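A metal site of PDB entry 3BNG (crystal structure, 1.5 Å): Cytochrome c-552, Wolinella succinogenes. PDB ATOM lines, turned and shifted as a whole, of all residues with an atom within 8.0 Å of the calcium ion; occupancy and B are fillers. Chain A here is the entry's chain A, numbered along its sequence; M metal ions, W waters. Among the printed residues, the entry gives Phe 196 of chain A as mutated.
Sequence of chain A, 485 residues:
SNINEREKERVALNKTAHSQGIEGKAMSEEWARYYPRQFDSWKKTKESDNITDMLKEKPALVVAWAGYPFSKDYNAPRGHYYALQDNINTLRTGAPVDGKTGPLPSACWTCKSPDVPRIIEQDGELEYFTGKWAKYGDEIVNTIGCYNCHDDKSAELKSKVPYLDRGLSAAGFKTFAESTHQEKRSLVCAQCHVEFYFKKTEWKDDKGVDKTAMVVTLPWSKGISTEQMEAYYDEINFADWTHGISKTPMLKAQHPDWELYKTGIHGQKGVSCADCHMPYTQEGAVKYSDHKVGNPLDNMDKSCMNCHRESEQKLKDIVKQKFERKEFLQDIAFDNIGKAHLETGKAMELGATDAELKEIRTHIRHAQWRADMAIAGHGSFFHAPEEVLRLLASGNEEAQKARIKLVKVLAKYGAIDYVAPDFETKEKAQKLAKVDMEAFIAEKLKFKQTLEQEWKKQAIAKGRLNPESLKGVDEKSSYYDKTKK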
ATOM      1  N   TYR A  68       5.850 -14.092  12.974  1.00  0.00           N
ATOM      2  CA  TYR A  68       5.756 -15.143  11.969  1.00  0.00           C
ATOM      3  C   TYR A  68       6.092 -16.487  12.628  1.00  0.00           C
ATOM      4  O   TYR A  68       6.837 -16.512  13.626  1.00  0.00           O
ATOM      5  CB  TYR A  68       6.775 -14.844  10.846  1.00  0.00           C
ATOM      6  CG  TYR A  68       6.528 -15.567   9.541  1.00  0.00           C
ATOM      7  CD1 TYR A  68       5.337 -15.409   8.831  1.00  0.00           C
ATOM      8  CD2 TYR A  68       7.523 -16.387   8.967  1.00  0.00           C
ATOM      9  CE1 TYR A  68       5.134 -16.085   7.625  1.00  0.00           C
ATOM     10  CE2 TYR A  68       7.321 -17.081   7.787  1.00  0.00           C
ATOM     11  CZ  TYR A  68       6.141 -16.915   7.112  1.00  0.00           C
ATOM     12  OH  TYR A  68       5.983 -17.589   5.914  1.00  0.00           O
ATOM     13  N   VAL A 194      13.473 -25.447  -3.117  1.00  0.00           N
ATOM     14  CA  VAL A 194      13.335 -24.160  -3.806  1.00  0.00           C
ATOM     15  C   VAL A 194      12.571 -23.189  -2.907  1.00  0.00           C
ATOM     16  O   VAL A 194      11.933 -23.615  -1.928  1.00  0.00           O
ATOM     17  CB  VAL A 194      12.579 -24.323  -5.170  1.00  0.00           C
ATOM     18  CG1 VAL A 194      13.450 -25.051  -6.191  1.00  0.00           C
ATOM     19  CG2 VAL A 194      11.230 -25.063  -4.977  1.00  0.00           C
ATOM     20  N   GLU A 195      12.694 -21.902  -3.215  1.00  0.00           N
ATOM     21  CA  GLU A 195      11.917 -20.856  -2.579  1.00  0.00           C
ATOM     22  C   GLU A 195      10.515 -20.795  -3.187  1.00  0.00           C
ATOM     23  O   GLU A 195      10.317 -20.965  -4.387  1.00  0.00           O
ATOM     24  CB  GLU A 195      12.650 -19.519  -2.691  1.00  0.00           C
ATOM     25  CG  GLU A 195      11.812 -18.226  -2.815  1.00  0.00           C
ATOM     26  CD  GLU A 195      10.955 -17.890  -1.612  1.00  0.00           C
ATOM     27  OE1 GLU A 195      11.124 -18.534  -0.557  1.00  0.00           O
ATOM     28  OE2 GLU A 195      10.113 -16.971  -1.714  1.00  0.00           O
ATOM     29  N   PHE A 196       9.526 -20.504  -2.343  1.00  0.00           N
ATOM     30  CA  PHE A 196       8.161 -20.519  -2.790  1.00  0.00           C
ATOM     31  C   PHE A 196       7.355 -19.491  -1.989  1.00  0.00           C
ATOM     32  O   PHE A 196       7.801 -18.946  -0.959  1.00  0.00           O
ATOM     33  CB  PHE A 196       7.564 -21.923  -2.597  1.00  0.00           C
ATOM     34  CG  PHE A 196       7.442 -22.295  -1.140  1.00  0.00           C
ATOM     35  CD1 PHE A 196       8.506 -22.862  -0.461  1.00  0.00           C
ATOM     36  CD2 PHE A 196       6.296 -21.930  -0.423  1.00  0.00           C
ATOM     37  CE1 PHE A 196       8.419 -23.148   0.907  1.00  0.00           C
ATOM     38  CE2 PHE A 196       6.187 -22.197   0.938  1.00  0.00           C
ATOM     39  CZ  PHE A 196       7.261 -22.828   1.606  1.00  0.00           C
ATOM     40  N   TYR A 197       6.170 -19.235  -2.491  1.00  0.00           N
ATOM     41  CA  TYR A 197       5.152 -18.577  -1.682  1.00  0.00           C
ATOM     42  C   TYR A 197       3.791 -19.208  -1.981  1.00  0.00           C
ATOM     43  O   TYR A 197       3.676 -20.104  -2.846  1.00  0.00           O
ATOM     44  CB  TYR A 197       5.123 -17.083  -1.963  1.00  0.00           C
ATOM     45  CG  TYR A 197       4.533 -16.673  -3.289  1.00  0.00           C
ATOM     46  CD1 TYR A 197       5.265 -16.788  -4.468  1.00  0.00           C
ATOM     47  CD2 TYR A 197       3.263 -16.072  -3.338  1.00  0.00           C
ATOM     48  CE1 TYR A 197       4.709 -16.353  -5.691  1.00  0.00           C
ATOM     49  CE2 TYR A 197       2.713 -15.642  -4.529  1.00  0.00           C
ATOM     50  CZ  TYR A 197       3.437 -15.783  -5.695  1.00  0.00           C
ATOM     51  OH  TYR A 197       2.880 -15.337  -6.876  1.00  0.00           O
ATOM     52  N   PHE A 198       2.815 -18.842  -1.164  1.00  0.00           N
ATOM     53  CA  PHE A 198       1.435 -19.292  -1.382  1.00  0.00           C
ATOM     54  C   PHE A 198       0.597 -18.225  -2.045  1.00  0.00           C
ATOM     55  O   PHE A 198       0.452 -17.125  -1.501  1.00  0.00           O
ATOM     56  CB  PHE A 198       0.745 -19.676  -0.071  1.00  0.00           C
ATOM     57  CG  PHE A 198       1.431 -20.797   0.706  1.00  0.00           C
ATOM     58  CD1 PHE A 198       2.267 -21.719   0.060  1.00  0.00           C
ATOM     59  CD2 PHE A 198       1.177 -20.962   2.065  1.00  0.00           C
ATOM     60  CE1 PHE A 198       2.867 -22.795   0.785  1.00  0.00           C
ATOM     61  CE2 PHE A 198       1.768 -22.001   2.787  1.00  0.00           C
ATOM     62  CZ  PHE A 198       2.611 -22.936   2.145  1.00  0.00           C
ATOM     63  N   THR A 217       3.686 -21.575  -5.258  1.00  0.00           N
ATOM     64  CA  THR A 217       4.077 -20.839  -6.454  1.00  0.00           C
ATOM     65  C   THR A 217       5.522 -20.441  -6.308  1.00  0.00           C
ATOM     66  O   THR A 217       5.953 -20.005  -5.220  1.00  0.00           O
ATOM     67  CB  THR A 217       3.218 -19.577  -6.607  1.00  0.00           C
ATOM     68  OG1 THR A 217       1.843 -19.931  -6.535  1.00  0.00           O
ATOM     69  CG2 THR A 217       3.489 -18.834  -7.919  1.00  0.00           C
ATOM     70  N   PRO A 219       8.443 -17.937  -7.236  1.00  0.00           N
ATOM     71  CA  PRO A 219       8.423 -16.516  -7.672  1.00  0.00           C
ATOM     72  C   PRO A 219       9.497 -16.241  -8.721  1.00  0.00           C
ATOM     73  O   PRO A 219      10.308 -15.330  -8.552  1.00  0.00           O
ATOM     74  CB  PRO A 219       8.726 -15.774  -6.378  1.00  0.00           C
ATOM     75  CG  PRO A 219       9.685 -16.757  -5.660  1.00  0.00           C
ATOM     76  CD  PRO A 219       9.207 -18.134  -5.977  1.00  0.00           C
ATOM     77  N   MET A 229      13.789 -12.059  -7.825  1.00  0.00           N
ATOM     78  CA  MET A 229      12.627 -12.433  -7.000  1.00  0.00           C
ATOM     79  C   MET A 229      12.157 -11.272  -6.131  1.00  0.00           C
ATOM     80  O   MET A 229      10.951 -11.115  -5.901  1.00  0.00           O
ATOM     81  CB  MET A 229      12.933 -13.625  -6.105  1.00  0.00           C
ATOM     82  CG  MET A 229      13.448 -14.848  -6.868  1.00  0.00           C
ATOM     83  SD  MET A 229      13.511 -16.198  -5.643  1.00  0.00           S
ATOM     84  CE  MET A 229      14.647 -17.300  -6.392  1.00  0.00           C
ATOM     85  N   TYR A 233       8.311  -9.819  -6.138  1.00  0.00           N
ATOM     86  CA  TYR A 233       7.468  -9.666  -4.958  1.00  0.00           C
ATOM     87  C   TYR A 233       7.075  -8.211  -4.725  1.00  0.00           C
ATOM     88  O   TYR A 233       5.970  -7.922  -4.294  1.00  0.00           O
ATOM     89  CB  TYR A 233       8.221 -10.195  -3.748  1.00  0.00           C
ATOM     90  CG  TYR A 233       8.196 -11.714  -3.565  1.00  0.00           C
ATOM     91  CD1 TYR A 233       6.994 -12.430  -3.660  1.00  0.00           C
ATOM     92  CD2 TYR A 233       9.379 -12.420  -3.277  1.00  0.00           C
ATOM     93  CE1 TYR A 233       6.952 -13.825  -3.445  1.00  0.00           C
ATOM     94  CE2 TYR A 233       9.370 -13.816  -3.076  1.00  0.00           C
ATOM     95  CZ  TYR A 233       8.149 -14.517  -3.168  1.00  0.00           C
ATOM     96  OH  TYR A 233       8.105 -15.887  -2.953  1.00  0.00           O
ATOM     97  N   PHE A 238       3.653  -7.973  -2.536  1.00  0.00           N
ATOM     98  CA  PHE A 238       3.460  -9.154  -1.673  1.00  0.00           C
ATOM     99  C   PHE A 238       4.167  -9.034  -0.335  1.00  0.00           C
ATOM    100  O   PHE A 238       5.298  -8.538  -0.284  1.00  0.00           O
ATOM    101  CB  PHE A 238       3.929 -10.430  -2.386  1.00  0.00           C
ATOM    102  CG  PHE A 238       3.558 -11.693  -1.660  1.00  0.00           C
ATOM    103  CD1 PHE A 238       2.264 -12.203  -1.704  1.00  0.00           C
ATOM    104  CD2 PHE A 238       4.525 -12.414  -0.948  1.00  0.00           C
ATOM    105  CE1 PHE A 238       1.924 -13.365  -1.034  1.00  0.00           C
ATOM    106  CE2 PHE A 238       4.175 -13.577  -0.264  1.00  0.00           C
ATOM    107  CZ  PHE A 238       2.889 -14.057  -0.309  1.00  0.00           C
ATOM    108  N   ASP A 240       4.759 -11.833   3.110  1.00  0.00           N
ATOM    109  CA  ASP A 240       4.435 -13.028   3.863  1.00  0.00           C
ATOM    110  C   ASP A 240       3.805 -12.735   5.253  1.00  0.00           C
ATOM    111  O   ASP A 240       2.952 -13.491   5.723  1.00  0.00           O
ATOM    112  CB  ASP A 240       5.684 -13.886   4.019  1.00  0.00           C
ATOM    113  CG  ASP A 240       6.060 -14.578   2.731  1.00  0.00           C
ATOM    114  OD1 ASP A 240       5.306 -15.496   2.338  1.00  0.00           O
ATOM    115  OD2 ASP A 240       7.086 -14.201   2.122  1.00  0.00           O
ATOM    116  N   LEU A 251       9.198 -10.350   3.610  1.00  0.00           N
ATOM    117  CA  LEU A 251       9.287 -11.561   2.765  1.00  0.00           C
ATOM    118  C   LEU A 251      10.085 -12.620   3.506  1.00  0.00           C
ATOM    119  O   LEU A 251      11.163 -12.340   4.069  1.00  0.00           O
ATOM    120  CB  LEU A 251       9.992 -11.225   1.460  1.00  0.00           C
ATOM    121  CG  LEU A 251       9.296 -10.200   0.548  1.00  0.00           C
ATOM    122  CD1 LEU A 251      10.244  -9.784  -0.551  1.00  0.00           C
ATOM    123  CD2 LEU A 251       7.985 -10.769  -0.008  1.00  0.00           C
ATOM    124  N   LYS A 252       9.566 -13.834   3.480  1.00  0.00           N
ATOM    125  CA  LYS A 252      10.285 -15.000   4.036  1.00  0.00           C
ATOM    126  C   LYS A 252      10.966 -15.820   2.924  1.00  0.00           C
ATOM    127  O   LYS A 252      10.318 -16.289   1.971  1.00  0.00           O
ATOM    128  CB  LYS A 252       9.326 -15.949   4.768  1.00  0.00           C
ATOM    129  CG  LYS A 252      10.040 -17.070   5.487  1.00  0.00           C
ATOM    130  CD  LYS A 252      10.707 -16.583   6.781  1.00  0.00           C
ATOM    131  CE  LYS A 252      11.642 -17.638   7.356  1.00  0.00           C
ATOM    132  NZ  LYS A 252      12.825 -17.871   6.479  1.00  0.00           N
ATOM    133  N   ALA A 253      12.259 -16.040   3.053  1.00  0.00           N
ATOM    134  CA  ALA A 253      12.964 -16.928   2.122  1.00  0.00           C
ATOM    135  C   ALA A 253      12.831 -18.336   2.667  1.00  0.00           C
ATOM    136  O   ALA A 253      12.977 -18.542   3.859  1.00  0.00           O
ATOM    137  CB  ALA A 253      14.460 -16.546   2.053  1.00  0.00           C
ATOM    138  N   GLN A 254      12.555 -19.312   1.813  1.00  0.00           N
ATOM    139  CA  GLN A 254      12.625 -20.713   2.275  1.00  0.00           C
ATOM    140  C   GLN A 254      13.582 -21.492   1.373  1.00  0.00           C
ATOM    141  O   GLN A 254      13.407 -21.540   0.141  1.00  0.00           O
ATOM    142  CB  GLN A 254      11.231 -21.373   2.254  1.00  0.00           C
ATOM    143  CG  GLN A 254      10.293 -20.984   3.396  1.00  0.00           C
ATOM    144  CD  GLN A 254       9.311 -19.894   2.971  1.00  0.00           C
ATOM    145  OE1 GLN A 254       9.508 -19.225   1.956  1.00  0.00           O
ATOM    146  NE2 GLN A 254       8.282 -19.687   3.779  1.00  0.00           N
ATOM    147  N   HIS A 255      14.623 -22.074   1.982  1.00  0.00           N
ATOM    148  CA  HIS A 255      15.501 -23.022   1.286  1.00  0.00           C
ATOM    149  C   HIS A 255      15.523 -22.888  -0.247  1.00  0.00           C
ATOM    150  O   HIS A 255      15.075 -23.791  -0.980  1.00  0.00           O
ATOM    151  CB  HIS A 255      15.146 -24.473   1.683  1.00  0.00           C
ATOM    152  CG  HIS A 255      13.667 -24.747   1.715  1.00  0.00           C
ATOM    153  ND1 HIS A 255      12.859 -24.695   0.591  1.00  0.00           N
ATOM    154  CD2 HIS A 255      12.845 -25.051   2.750  1.00  0.00           C
ATOM    155  CE1 HIS A 255      11.614 -24.953   0.941  1.00  0.00           C
ATOM    156  NE2 HIS A 255      11.578 -25.177   2.249  1.00  0.00           N
ATOM    157  N   TRP A 369      15.189  -9.824   3.194  1.00  0.00           N
ATOM    158  CA  TRP A 369      15.012 -10.734   2.030  1.00  0.00           C
ATOM    159  C   TRP A 369      16.357 -11.272   1.543  1.00  0.00           C
ATOM    160  O   TRP A 369      16.508 -12.485   1.317  1.00  0.00           O
ATOM    161  CB  TRP A 369      14.254 -10.027   0.896  1.00  0.00           C
ATOM    162  CG  TRP A 369      14.214 -10.841  -0.319  1.00  0.00           C
ATOM    163  CD1 TRP A 369      14.788 -10.519  -1.535  1.00  0.00           C
ATOM    164  CD2 TRP A 369      13.543 -12.102  -0.497  1.00  0.00           C
ATOM    165  NE1 TRP A 369      14.528 -11.538  -2.451  1.00  0.00           N
ATOM    166  CE2 TRP A 369      13.763 -12.512  -1.838  1.00  0.00           C
ATOM    167  CE3 TRP A 369      12.775 -12.935   0.348  1.00  0.00           C
ATOM    168  CZ2 TRP A 369      13.242 -13.700  -2.341  1.00  0.00           C
ATOM    169  CZ3 TRP A 369      12.275 -14.117  -0.148  1.00  0.00           C
ATOM    170  CH2 TRP A 369      12.505 -14.502  -1.481  1.00  0.00           C
ATOM    171  N   ASP A 372      18.200 -13.439   4.242  1.00  0.00           N
ATOM    172  CA  ASP A 372      17.499 -14.700   4.496  1.00  0.00           C
ATOM    173  C   ASP A 372      17.715 -15.592   3.266  1.00  0.00           C
ATOM    174  O   ASP A 372      18.019 -16.795   3.408  1.00  0.00           O
ATOM    175  CB  ASP A 372      15.988 -14.441   4.725  1.00  0.00           C
ATOM    176  CG  ASP A 372      15.257 -15.600   5.470  1.00  0.00           C
ATOM    177  OD1 ASP A 372      15.908 -16.583   5.892  1.00  0.00           O
ATOM    178  OD2 ASP A 372      13.992 -15.493   5.558  1.00  0.00           O
ATOM    179  N   MET A 373      17.563 -15.038   2.044  1.00  0.00           N
ATOM    180  CA  MET A 373      17.855 -15.855   0.833  1.00  0.00           C
ATOM    181  C   MET A 373      19.301 -16.420   0.892  1.00  0.00           C
ATOM    182  O   MET A 373      19.560 -17.530   0.405  1.00  0.00           O
ATOM    183  CB  MET A 373      17.657 -15.057  -0.442  1.00  0.00           C
ATOM    184  CG  MET A 373      16.179 -14.960  -0.865  1.00  0.00           C
ATOM    185  SD  MET A 373      15.572 -16.530  -1.506  1.00  0.00           S
ATOM    186  CE  MET A 373      16.624 -16.689  -2.965  1.00  0.00           C
HETATM  187 CA    CA M   1       9.037 -17.579   0.439  1.00  0.00          CA
HETATM  188  O   HOH W   1       7.000 -17.679   1.742  1.00  0.00           O
HETATM  189  O   HOH W   2       7.923 -15.474  -0.012  1.00  0.00           O
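The backbone NH (N) of Phe 238 lies within hydrogen-bond range of the backbone carbonyl oxygen (O) of Tyr 233, 2.9 Å away. OH of Tyr 233 sits close to OE2 of Glu 195 (2.6 Å). N of Lys 252 sits at hydrogen-bond distance from OD2 of Asp 240 (2.9 Å). The side-chain carboxylate (OD2) of Asp 372 is in salt-bridge range of the side-chain amino group (NZ) of Lys 252 (2.8 Å).
Tyr 233 touches the calcium ion. The nearest printed residue that does not touch the calcium ion is Asp 240 (4.2 Å).
The calcium ion is bound by the side-chain amide oxygen (OE1) of Gln 254, the backbone carbonyl oxygen (O) of Phe 196, the backbone carbonyl oxygen (O) of Lys 252, water W1, water W2, the side-chain carboxylate (OE2) of Glu 195 and the side-chain carboxylate (OE1) of Glu 195.
Water W1 bridges OD1 of Asp 240 (2.8 Å) and NE2 of Gln 254 (3.1 Å). Water W2 lies within hydrogen-bond range of OD2 of Asp 240 (2.6 Å) and OH of Tyr 233 (3.0 Å).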
